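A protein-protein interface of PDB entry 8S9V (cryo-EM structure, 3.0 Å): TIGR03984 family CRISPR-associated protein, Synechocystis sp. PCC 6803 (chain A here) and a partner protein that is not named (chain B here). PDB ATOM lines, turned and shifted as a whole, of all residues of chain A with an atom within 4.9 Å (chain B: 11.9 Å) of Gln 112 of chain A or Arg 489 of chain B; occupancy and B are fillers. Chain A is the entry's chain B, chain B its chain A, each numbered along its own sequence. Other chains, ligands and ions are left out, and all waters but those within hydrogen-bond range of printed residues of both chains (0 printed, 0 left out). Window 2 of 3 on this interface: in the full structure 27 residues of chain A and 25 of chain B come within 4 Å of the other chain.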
ATOM      1  N   LYS A   9      -5.485 -18.019  11.155  1.00  0.00           N
ATOM      2  CA  LYS A   9      -4.480 -17.006  10.884  1.00  0.00           C
ATOM      3  C   LYS A   9      -3.980 -17.158   9.462  1.00  0.00           C
ATOM      4  O   LYS A   9      -3.786 -18.269   8.993  1.00  0.00           O
ATOM      5  CB  LYS A   9      -3.328 -17.136  11.864  1.00  0.00           C
ATOM      6  CG  LYS A   9      -3.751 -17.031  13.296  1.00  0.00           C
ATOM      7  CD  LYS A   9      -2.589 -17.238  14.227  1.00  0.00           C
ATOM      8  CE  LYS A   9      -1.677 -16.049  14.214  1.00  0.00           C
ATOM      9  NZ  LYS A   9      -2.272 -14.937  14.997  1.00  0.00           N
ATOM     10  N   ASN A  10      -3.799 -16.050   8.756  1.00  0.00           N
ATOM     11  CA  ASN A  10      -3.328 -16.074   7.381  1.00  0.00           C
ATOM     12  C   ASN A  10      -1.904 -15.545   7.268  1.00  0.00           C
ATOM     13  O   ASN A  10      -1.583 -14.499   7.837  1.00  0.00           O
ATOM     14  CB  ASN A  10      -4.262 -15.258   6.502  1.00  0.00           C
ATOM     15  CG  ASN A  10      -5.623 -15.851   6.441  1.00  0.00           C
ATOM     16  OD1 ASN A  10      -5.782 -17.050   6.631  1.00  0.00           O
ATOM     17  ND2 ASN A  10      -6.625 -15.023   6.200  1.00  0.00           N
ATOM     18  N   LEU A  11      -1.050 -16.286   6.570  1.00  0.00           N
ATOM     19  CA  LEU A  11       0.190 -15.759   6.014  1.00  0.00           C
ATOM     20  C   LEU A  11      -0.093 -15.393   4.561  1.00  0.00           C
ATOM     21  O   LEU A  11      -0.294 -16.279   3.728  1.00  0.00           O
ATOM     22  CB  LEU A  11       1.315 -16.780   6.129  1.00  0.00           C
ATOM     23  CG  LEU A  11       2.673 -16.502   5.498  1.00  0.00           C
ATOM     24  CD1 LEU A  11       3.324 -15.326   6.154  1.00  0.00           C
ATOM     25  CD2 LEU A  11       3.549 -17.705   5.668  1.00  0.00           C
ATOM     26  N   HIS A  13       0.800 -14.059   0.780  1.00  0.00           N
ATOM     27  CA  HIS A  13       1.928 -14.045  -0.142  1.00  0.00           C
ATOM     28  C   HIS A  13       1.496 -13.612  -1.533  1.00  0.00           C
ATOM     29  O   HIS A  13       0.443 -14.027  -2.016  1.00  0.00           O
ATOM     30  CB  HIS A  13       2.581 -15.412  -0.272  1.00  0.00           C
ATOM     31  CG  HIS A  13       1.612 -16.513  -0.540  1.00  0.00           C
ATOM     32  ND1 HIS A  13       1.068 -16.729  -1.786  1.00  0.00           N
ATOM     33  CD2 HIS A  13       1.115 -17.482   0.259  1.00  0.00           C
ATOM     34  CE1 HIS A  13       0.261 -17.771  -1.738  1.00  0.00           C
ATOM     35  NE2 HIS A  13       0.269 -18.244  -0.507  1.00  0.00           N
ATOM     36  N   HIS A  15       2.546 -13.013  -5.630  1.00  0.00           N
ATOM     37  CA  HIS A  15       3.440 -13.507  -6.671  1.00  0.00           C
ATOM     38  C   HIS A  15       3.386 -12.624  -7.900  1.00  0.00           C
ATOM     39  O   HIS A  15       2.317 -12.157  -8.296  1.00  0.00           O
ATOM     40  CB  HIS A  15       3.111 -14.932  -7.103  1.00  0.00           C
ATOM     41  CG  HIS A  15       2.946 -15.890  -5.973  1.00  0.00           C
ATOM     42  ND1 HIS A  15       3.987 -16.650  -5.495  1.00  0.00           N
ATOM     43  CD2 HIS A  15       1.867 -16.213  -5.226  1.00  0.00           C
ATOM     44  CE1 HIS A  15       3.556 -17.404  -4.502  1.00  0.00           C
ATOM     45  NE2 HIS A  15       2.273 -17.156  -4.318  1.00  0.00           N
ATOM     46  N   ARG A  83      11.207 -12.085  -1.650  1.00  0.00           N
ATOM     47  CA  ARG A  83      12.141 -13.034  -2.229  1.00  0.00           C
ATOM     48  C   ARG A  83      12.077 -12.939  -3.736  1.00  0.00           C
ATOM     49  O   ARG A  83      11.001 -12.789  -4.308  1.00  0.00           O
ATOM     50  CB  ARG A  83      11.835 -14.452  -1.813  1.00  0.00           C
ATOM     51  CG  ARG A  83      11.847 -14.674  -0.350  1.00  0.00           C
ATOM     52  CD  ARG A  83      11.547 -16.095  -0.074  1.00  0.00           C
ATOM     53  NE  ARG A  83      11.295 -16.330   1.330  1.00  0.00           N
ATOM     54  CZ  ARG A  83      10.363 -17.149   1.783  1.00  0.00           C
ATOM     55  NH1 ARG A  83      10.094 -17.200   3.071  1.00  0.00           N
ATOM     56  NH2 ARG A  83       9.608 -17.807   0.927  1.00  0.00           N
ATOM     57  N   VAL A  95       8.095 -13.082  -4.879  1.00  0.00           N
ATOM     58  CA  VAL A  95       7.081 -13.442  -3.905  1.00  0.00           C
ATOM     59  C   VAL A  95       7.309 -12.605  -2.666  1.00  0.00           C
ATOM     60  O   VAL A  95       8.393 -12.655  -2.081  1.00  0.00           O
ATOM     61  CB  VAL A  95       7.136 -14.932  -3.565  1.00  0.00           C
ATOM     62  CG1 VAL A  95       6.047 -15.283  -2.607  1.00  0.00           C
ATOM     63  CG2 VAL A  95       6.984 -15.728  -4.825  1.00  0.00           C
ATOM     64  N   LEU A  97       5.984 -11.979   1.195  1.00  0.00           N
ATOM     65  CA  LEU A  97       5.246 -12.648   2.259  1.00  0.00           C
ATOM     66  C   LEU A  97       5.009 -11.696   3.410  1.00  0.00           C
ATOM     67  O   LEU A  97       5.956 -11.100   3.925  1.00  0.00           O
ATOM     68  CB  LEU A  97       6.009 -13.852   2.793  1.00  0.00           C
ATOM     69  CG  LEU A  97       6.396 -14.974   1.863  1.00  0.00           C
ATOM     70  CD1 LEU A  97       7.809 -14.801   1.420  1.00  0.00           C
ATOM     71  CD2 LEU A  97       6.275 -16.221   2.659  1.00  0.00           C
ATOM     72  N   GLY A 110      -2.276 -14.186  -2.744  1.00  0.00           N
ATOM     73  CA  GLY A 110      -2.804 -15.418  -2.202  1.00  0.00           C
ATOM     74  C   GLY A 110      -2.559 -15.466  -0.709  1.00  0.00           C
ATOM     75  O   GLY A 110      -1.972 -14.553  -0.130  1.00  0.00           O
ATOM     76  N   LEU A 111      -3.017 -16.541  -0.075  1.00  0.00           N
ATOM     77  CA  LEU A 111      -2.688 -16.738   1.328  1.00  0.00           C
ATOM     78  C   LEU A 111      -2.774 -18.215   1.665  1.00  0.00           C
ATOM     79  O   LEU A 111      -3.384 -19.000   0.938  1.00  0.00           O
ATOM     80  CB  LEU A 111      -3.617 -15.932   2.230  1.00  0.00           C
ATOM     81  CG  LEU A 111      -5.073 -16.372   2.245  1.00  0.00           C
ATOM     82  CD1 LEU A 111      -5.301 -17.393   3.326  1.00  0.00           C
ATOM     83  CD2 LEU A 111      -5.960 -15.172   2.458  1.00  0.00           C
ATOM     84  N   GLN A 112      -2.159 -18.578   2.788  1.00  0.00           N
ATOM     85  CA  GLN A 112      -2.380 -19.860   3.436  1.00  0.00           C
ATOM     86  C   GLN A 112      -2.537 -19.685   4.935  1.00  0.00           C
ATOM     87  O   GLN A 112      -1.802 -18.914   5.550  1.00  0.00           O
ATOM     88  CB  GLN A 112      -1.212 -20.790   3.158  1.00  0.00           C
ATOM     89  CG  GLN A 112      -1.411 -22.170   3.675  1.00  0.00           C
ATOM     90  CD  GLN A 112      -0.379 -23.111   3.147  1.00  0.00           C
ATOM     91  OE1 GLN A 112       0.547 -22.697   2.458  1.00  0.00           O
ATOM     92  NE2 GLN A 112      -0.525 -24.389   3.464  1.00  0.00           N
ATOM     93  N   GLU A 113      -3.470 -20.423   5.524  1.00  0.00           N
ATOM     94  CA  GLU A 113      -3.609 -20.455   6.974  1.00  0.00           C
ATOM     95  C   GLU A 113      -2.428 -21.145   7.630  1.00  0.00           C
ATOM     96  O   GLU A 113      -1.826 -22.057   7.069  1.00  0.00           O
ATOM     97  CB  GLU A 113      -4.904 -21.150   7.380  1.00  0.00           C
ATOM     98  CG  GLU A 113      -6.148 -20.357   7.049  1.00  0.00           C
ATOM     99  CD  GLU A 113      -7.407 -20.984   7.603  1.00  0.00           C
ATOM    100  OE1 GLU A 113      -7.552 -22.219   7.500  1.00  0.00           O
ATOM    101  OE2 GLU A 113      -8.251 -20.243   8.151  1.00  0.00           O
ATOM    102  N   PHE A 114      -2.089 -20.691   8.832  1.00  0.00           N
ATOM    103  CA  PHE A 114      -1.133 -21.391   9.671  1.00  0.00           C
ATOM    104  C   PHE A 114      -1.666 -21.502  11.093  1.00  0.00           C
ATOM    105  O   PHE A 114      -2.426 -20.653  11.555  1.00  0.00           O
ATOM    106  CB  PHE A 114       0.233 -20.705   9.622  1.00  0.00           C
ATOM    107  CG  PHE A 114       0.273 -19.357  10.256  1.00  0.00           C
ATOM    108  CD1 PHE A 114       0.584 -19.213  11.587  1.00  0.00           C
ATOM    109  CD2 PHE A 114      -0.002 -18.233   9.519  1.00  0.00           C
ATOM    110  CE1 PHE A 114       0.629 -17.973  12.160  1.00  0.00           C
ATOM    111  CE2 PHE A 114       0.034 -17.003  10.089  1.00  0.00           C
ATOM    112  CZ  PHE A 114       0.350 -16.871  11.411  1.00  0.00           C
ATOM    113  N   ILE A 183       5.413 -24.413   7.250  1.00  0.00           N
ATOM    114  CA  ILE A 183       5.153 -24.074   5.861  1.00  0.00           C
ATOM    115  C   ILE A 183       5.972 -22.916   5.305  1.00  0.00           C
ATOM    116  O   ILE A 183       6.014 -22.740   4.080  1.00  0.00           O
ATOM    117  CB  ILE A 183       3.675 -23.713   5.708  1.00  0.00           C
ATOM    118  CG1 ILE A 183       3.346 -22.582   6.671  1.00  0.00           C
ATOM    119  CG2 ILE A 183       2.823 -24.896   6.009  1.00  0.00           C
ATOM    120  CD1 ILE A 183       2.147 -21.792   6.277  1.00  0.00           C
ATOM    121  N   ASP A 184       6.591 -22.100   6.154  1.00  0.00           N
ATOM    122  CA  ASP A 184       7.539 -21.100   5.687  1.00  0.00           C
ATOM    123  C   ASP A 184       8.383 -20.675   6.873  1.00  0.00           C
ATOM    124  O   ASP A 184       8.017 -20.923   8.018  1.00  0.00           O
ATOM    125  CB  ASP A 184       6.813 -19.916   5.053  1.00  0.00           C
ATOM    126  CG  ASP A 184       7.714 -19.080   4.181  1.00  0.00           C
ATOM    127  OD1 ASP A 184       8.196 -19.609   3.161  1.00  0.00           O
ATOM    128  OD2 ASP A 184       7.920 -17.888   4.494  1.00  0.00           O
ATOM    129  N   LEU B 485      13.926 -28.643  -5.710  1.00  0.00           N
ATOM    130  CA  LEU B 485      12.806 -27.834  -6.149  1.00  0.00           C
ATOM    131  C   LEU B 485      12.507 -26.741  -5.146  1.00  0.00           C
ATOM    132  O   LEU B 485      12.692 -26.910  -3.945  1.00  0.00           O
ATOM    133  CB  LEU B 485      11.531 -28.647  -6.370  1.00  0.00           C
ATOM    134  CG  LEU B 485      11.361 -29.547  -7.583  1.00  0.00           C
ATOM    135  CD1 LEU B 485       9.942 -29.979  -7.635  1.00  0.00           C
ATOM    136  CD2 LEU B 485      11.686 -28.793  -8.824  1.00  0.00           C
ATOM    137  N   ARG B 486      12.045 -25.618  -5.667  1.00  0.00           N
ATOM    138  CA  ARG B 486      11.523 -24.533  -4.860  1.00  0.00           C
ATOM    139  C   ARG B 486      10.009 -24.598  -4.804  1.00  0.00           C
ATOM    140  O   ARG B 486       9.349 -24.781  -5.826  1.00  0.00           O
ATOM    141  CB  ARG B 486      11.961 -23.189  -5.420  1.00  0.00           C
ATOM    142  CG  ARG B 486      13.420 -22.990  -5.283  1.00  0.00           C
ATOM    143  CD  ARG B 486      13.849 -21.689  -5.815  1.00  0.00           C
ATOM    144  NE  ARG B 486      15.288 -21.612  -5.759  1.00  0.00           N
ATOM    145  CZ  ARG B 486      15.938 -20.860  -4.895  1.00  0.00           C
ATOM    146  NH1 ARG B 486      17.252 -20.748  -4.961  1.00  0.00           N
ATOM    147  NH2 ARG B 486      15.261 -20.177  -3.996  1.00  0.00           N
ATOM    148  N   GLY B 487       9.464 -24.413  -3.621  1.00  0.00           N
ATOM    149  CA  GLY B 487       8.041 -24.234  -3.514  1.00  0.00           C
ATOM    150  C   GLY B 487       7.629 -22.938  -4.160  1.00  0.00           C
ATOM    151  O   GLY B 487       8.448 -22.157  -4.633  1.00  0.00           O
ATOM    152  N   ASP B 488       6.325 -22.712  -4.218  1.00  0.00           N
ATOM    153  CA  ASP B 488       5.884 -21.448  -4.784  1.00  0.00           C
ATOM    154  C   ASP B 488       6.272 -20.250  -3.939  1.00  0.00           C
ATOM    155  O   ASP B 488       6.014 -19.123  -4.362  1.00  0.00           O
ATOM    156  CB  ASP B 488       4.376 -21.468  -5.025  1.00  0.00           C
ATOM    157  CG  ASP B 488       3.592 -21.692  -3.765  1.00  0.00           C
ATOM    158  OD1 ASP B 488       4.216 -22.035  -2.745  1.00  0.00           O
ATOM    159  OD2 ASP B 488       2.354 -21.514  -3.790  1.00  0.00           O
ATOM    160  N   ARG B 489       6.869 -20.451  -2.770  1.00  0.00           N
ATOM    161  CA  ARG B 489       7.471 -19.377  -2.000  1.00  0.00           C
ATOM    162  C   ARG B 489       8.962 -19.262  -2.231  1.00  0.00           C
ATOM    163  O   ARG B 489       9.644 -18.566  -1.482  1.00  0.00           O
ATOM    164  CB  ARG B 489       7.196 -19.579  -0.527  1.00  0.00           C
ATOM    165  CG  ARG B 489       5.749 -19.543  -0.223  1.00  0.00           C
ATOM    166  CD  ARG B 489       5.519 -19.715   1.238  1.00  0.00           C
ATOM    167  NE  ARG B 489       4.103 -19.813   1.471  1.00  0.00           N
ATOM    168  CZ  ARG B 489       3.484 -20.970   1.635  1.00  0.00           C
ATOM    169  NH1 ARG B 489       2.170 -21.042   1.581  1.00  0.00           N
ATOM    170  NH2 ARG B 489       4.201 -22.083   1.625  1.00  0.00           N
ATOM    171  N   LEU B 490       9.484 -19.942  -3.239  1.00  0.00           N
ATOM    172  CA  LEU B 490      10.889 -19.856  -3.595  1.00  0.00           C
ATOM    173  C   LEU B 490      11.834 -20.374  -2.528  1.00  0.00           C
ATOM    174  O   LEU B 490      13.049 -20.299  -2.710  1.00  0.00           O
ATOM    175  CB  LEU B 490      11.243 -18.419  -3.939  1.00  0.00           C
ATOM    176  CG  LEU B 490      10.329 -17.809  -4.983  1.00  0.00           C
ATOM    177  CD1 LEU B 490      10.773 -16.434  -5.269  1.00  0.00           C
ATOM    178  CD2 LEU B 490      10.377 -18.631  -6.217  1.00  0.00           C
ATOM    179  N   ASN B 491      11.331 -20.834  -1.397  1.00  0.00           N
ATOM    180  CA  ASN B 491      12.191 -21.664  -0.573  1.00  0.00           C
ATOM    181  C   ASN B 491      12.034 -23.123  -0.995  1.00  0.00           C
ATOM    182  O   ASN B 491      11.183 -23.468  -1.812  1.00  0.00           O
ATOM    183  CB  ASN B 491      11.885 -21.488   0.909  1.00  0.00           C
ATOM    184  CG  ASN B 491      10.432 -21.640   1.226  1.00  0.00           C
ATOM    185  OD1 ASN B 491       9.679 -22.237   0.471  1.00  0.00           O
ATOM    186  ND2 ASN B 491      10.024 -21.101   2.357  1.00  0.00           N
ATOM    187  N   PHE B 492      12.899 -23.982  -0.470  1.00  0.00           N
ATOM    188  CA  PHE B 492      12.986 -25.351  -0.965  1.00  0.00           C
ATOM    189  C   PHE B 492      11.958 -26.308  -0.371  1.00  0.00           C
ATOM    190  O   PHE B 492      12.066 -27.512  -0.593  1.00  0.00           O
ATOM    191  CB  PHE B 492      14.395 -25.900  -0.778  1.00  0.00           C
ATOM    192  CG  PHE B 492      15.400 -25.267  -1.671  1.00  0.00           C
ATOM    193  CD1 PHE B 492      15.528 -25.699  -2.963  1.00  0.00           C
ATOM    194  CD2 PHE B 492      16.195 -24.248  -1.245  1.00  0.00           C
ATOM    195  CE1 PHE B 492      16.426 -25.150  -3.804  1.00  0.00           C
ATOM    196  CE2 PHE B 492      17.106 -23.693  -2.098  1.00  0.00           C
ATOM    197  CZ  PHE B 492      17.214 -24.151  -3.381  1.00  0.00           C
ATOM    198  N   ASN B 493      10.941 -25.829   0.321  1.00  0.00           N
ATOM    199  CA  ASN B 493      10.004 -26.739   0.961  1.00  0.00           C
ATOM    200  C   ASN B 493       9.006 -27.354  -0.013  1.00  0.00           C
ATOM    201  O   ASN B 493       7.846 -27.561   0.345  1.00  0.00           O
ATOM    202  CB  ASN B 493       9.266 -26.020   2.088  1.00  0.00           C
ATOM    203  CG  ASN B 493       8.264 -25.018   1.583  1.00  0.00           C
ATOM    204  OD1 ASN B 493       7.960 -24.961   0.394  1.00  0.00           O
ATOM    205  ND2 ASN B 493       7.747 -24.207   2.488  1.00  0.00           N
ATOM    206  N   ALA B 494       9.420 -27.621  -1.243  1.00  0.00           N
ATOM    207  CA  ALA B 494       8.523 -28.257  -2.197  1.00  0.00           C
ATOM    208  C   ALA B 494       8.182 -29.679  -1.759  1.00  0.00           C
ATOM    209  O   ALA B 494       8.816 -30.262  -0.877  1.00  0.00           O
ATOM    210  CB  ALA B 494       9.138 -28.282  -3.588  1.00  0.00           C
ATOM    211  N   THR B 495       7.164 -30.237  -2.395  1.00  0.00           N
ATOM    212  CA  THR B 495       6.587 -31.530  -2.070  1.00  0.00           C
ATOM    213  C   THR B 495       6.424 -32.310  -3.360  1.00  0.00           C
ATOM    214  O   THR B 495       6.480 -31.739  -4.452  1.00  0.00           O
ATOM    215  CB  THR B 495       5.223 -31.403  -1.384  1.00  0.00           C
ATOM    216  OG1 THR B 495       4.265 -30.915  -2.324  1.00  0.00           O
ATOM    217  CG2 THR B 495       5.295 -30.431  -0.244  1.00  0.00           C
ATOM    218  N   ASP B 497       3.838 -33.251  -4.728  1.00  0.00           N
ATOM    219  CA  ASP B 497       2.782 -32.665  -5.543  1.00  0.00           C
ATOM    220  C   ASP B 497       3.246 -31.456  -6.337  1.00  0.00           C
ATOM    221  O   ASP B 497       2.699 -31.182  -7.409  1.00  0.00           O
ATOM    222  CB  ASP B 497       1.600 -32.273  -4.665  1.00  0.00           C
ATOM    223  CG  ASP B 497       0.803 -33.466  -4.209  1.00  0.00           C
ATOM    224  OD1 ASP B 497       0.633 -34.408  -5.014  1.00  0.00           O
ATOM    225  OD2 ASP B 497       0.335 -33.459  -3.053  1.00  0.00           O
ATOM    226  N   ASP B 498       4.220 -30.706  -5.829  1.00  0.00           N
ATOM    227  CA  ASP B 498       4.871 -29.694  -6.652  1.00  0.00           C
ATOM    228  C   ASP B 498       5.623 -30.320  -7.812  1.00  0.00           C
ATOM    229  O   ASP B 498       5.631 -29.779  -8.924  1.00  0.00           O
ATOM    230  CB  ASP B 498       5.821 -28.851  -5.810  1.00  0.00           C
ATOM    231  CG  ASP B 498       5.139 -28.208  -4.622  1.00  0.00           C
ATOM    232  OD1 ASP B 498       4.249 -27.361  -4.830  1.00  0.00           O
ATOM    233  OD2 ASP B 498       5.510 -28.532  -3.475  1.00  0.00           O
ATOM    234  N   LYS B 501       3.125 -31.239 -10.608  1.00  0.00           N
ATOM    235  CA  LYS B 501       2.824 -30.050 -11.394  1.00  0.00           C
ATOM    236  C   LYS B 501       3.993 -29.619 -12.262  1.00  0.00           C
ATOM    237  O   LYS B 501       3.796 -29.185 -13.399  1.00  0.00           O
ATOM    238  CB  LYS B 501       2.385 -28.911 -10.482  1.00  0.00           C
ATOM    239  CG  LYS B 501       0.961 -29.044 -10.010  1.00  0.00           C
ATOM    240  CD  LYS B 501       0.583 -27.916  -9.089  1.00  0.00           C
ATOM    241  CE  LYS B 501      -0.854 -28.051  -8.627  1.00  0.00           C
ATOM    242  NZ  LYS B 501      -1.260 -26.923  -7.744  1.00  0.00           N
ATOM    243  N   SER B 542      21.433 -23.454   2.361  1.00  0.00           N
ATOM    244  CA  SER B 542      21.171 -24.877   2.471  1.00  0.00           C
ATOM    245  C   SER B 542      20.185 -25.307   1.401  1.00  0.00           C
ATOM    246  O   SER B 542      19.146 -24.674   1.218  1.00  0.00           O
ATOM    247  CB  SER B 542      20.639 -25.188   3.853  1.00  0.00           C
ATOM    248  OG  SER B 542      20.535 -26.568   4.036  1.00  0.00           O
ATOM    249  N   ASP B 576      16.338 -26.651  -9.623  1.00  0.00           N
ATOM    250  CA  ASP B 576      17.401 -25.699  -9.328  1.00  0.00           C
ATOM    251  C   ASP B 576      18.787 -26.257  -9.633  1.00  0.00           C
ATOM    252  O   ASP B 576      19.057 -27.438  -9.439  1.00  0.00           O
ATOM    253  CB  ASP B 576      17.304 -25.256  -7.882  1.00  0.00           C
ATOM    254  CG  ASP B 576      17.462 -23.777  -7.729  1.00  0.00           C
ATOM    255  OD1 ASP B 576      16.712 -23.036  -8.394  1.00  0.00           O
ATOM    256  OD2 ASP B 576      18.313 -23.346  -6.932  1.00  0.00           O
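Of chain A, only His 13, Arg 83, Leu 97, Gln 112, Ile 183 and Asp 184 come within 4 Å of Arg 489 of chain B.
No residue of chain B comes within 4 Å of Asn 10 of chain A.
No residue of chain B comes within 4 Å of Leu 11 of chain A.
His 13 of chain A touches just one residue of chain B: Arg 489 (3.9 Å).
Arg 83 of chain A touches just these residues of chain B: Arg 489 (2.5 Å), Leu 490 (3.8 Å) and Asn 491 (3.6 Å).
Of chain B, only Asp 488 (3.6 Å) and Leu 490 (3.9 Å) come within 4 Å of Val 95 of chain A.
No residue of chain B comes within 4 Å of Gly 110 of chain A.
No residue of chain B comes within 4 Å of Leu 111 of chain A.
No residue of chain B comes within 4 Å of Glu 113 of chain A.
Phe 114 of chain A touches none of the printed residues of chain B.
Ile 183 of chain A touches two residues of chain B.
Asp 184 of chain A touches two residues of chain B.
Printed residues of chain B within 4 Å of His 15 of chain A: Asp 488.
Of the printed residues of chain A, Leu 490 of chain B touches Arg 83 (3.8 Å) and Val 95 (3.9 Å).
Of the printed residues of chain A, Asp 488 of chain B touches His 15 and Val 95.
Of the printed residues of chain A, Asn 491 of chain B touches Arg 83 (3.6 Å) and Asp 184 (2.5 Å).
Ser 542 of chain B touches none of the printed residues of chain A.
The nearest printed residue of chain A that does not touch Leu 490 of chain B is His 15 of chain A (6.5 Å).
Of the 15 printed residues of chain A, 8 touch a printed residue of chain B.
Printed residues of chain A that touch a printed residue of chain B: His 13, His 15, Arg 83, Val 95, Leu 97, Gln 112, Ile 183 and Asp 184.
Printed residues of chain B that touch a printed residue of chain A: Asp 488, Arg 489, Leu 490, Asn 491 and Asn 493.
Among the printed residues, no Asp or Glu carboxylate lies within 4 Å of a Lys or Arg side-chain nitrogen of the other chain.
His 13 of chain A touches Arg 489 of chain B.
Arg 83 of chain A touches Leu 490 of chain B (O to CD1, 3.8 Å).
Arg 83 of chain A touches Asn 491 of chain B.
O of Asp 488 of chain B touches CG2 of Val 95 of chain A, at 3.6 Å.
Val 95 of chain A touches Leu 490 of chain B.
Arg 489 of chain B touches Leu 97 of chain A (CD to CD2, 3.8 Å).
Asp 184 of chain A touches Arg 489 of chain B.
The side-chain amide oxygen (OD1) of Asn 491 of chain B sits close to the side-chain amide oxygen (OD1) of Asn 493 of chain B (3.2 Å).
A ring nitrogen (ND1) of His 13 of chain A sits at hydrogen-bond distance from a ring nitrogen (NE2) of His 15 of chain A (2.8 Å).
The backbone carbonyl oxygen (O) of Val 95 of chain A is in hydrogen-bond range of the backbone NH (N) of Arg 83 of chain A (2.9 Å).
The side-chain carboxylate of Asp 184 of chain A lies within salt-bridge range of the guanidinium group of Arg 83 of chain A (2.7 Å).
The backbone carbonyl oxygen (O) of His 13 of chain A is in hydrogen-bond range of the backbone NH (N) of Gly 110 of chain A (2.8 Å).
N of Leu 11 of chain A lies within hydrogen-bond range of O of Gln 112 of chain A (2.9 Å).
OE1 of Gln 112 of chain A is in hydrogen-bond range of NH1 of Arg 489 of chain B (2.5 Å).
The side-chain amide nitrogen (ND2) of Asn 493 of chain B lies within hydrogen-bond range of the backbone carbonyl oxygen (O) of Ile 183 of chain A.
The backbone carbonyl oxygen (O) of Asp 488 of chain B sits close to a ring nitrogen (ND1) of His 15 of chain A.
The side-chain amide nitrogen (ND2) of Asn 491 of chain B is in hydrogen-bond range of the side-chain carboxylate (OD1) of Asp 184 of chain A, 2.5 Å away.
The guanidinium group (NH2) of Arg 489 of chain B lies within hydrogen-bond range of the backbone carbonyl oxygen (O) of Ile 183 of chain A, 3.1 Å away.
NH2 of Arg 83 of chain A lies within hydrogen-bond range of O of Arg 489 of chain B (2.5 Å).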
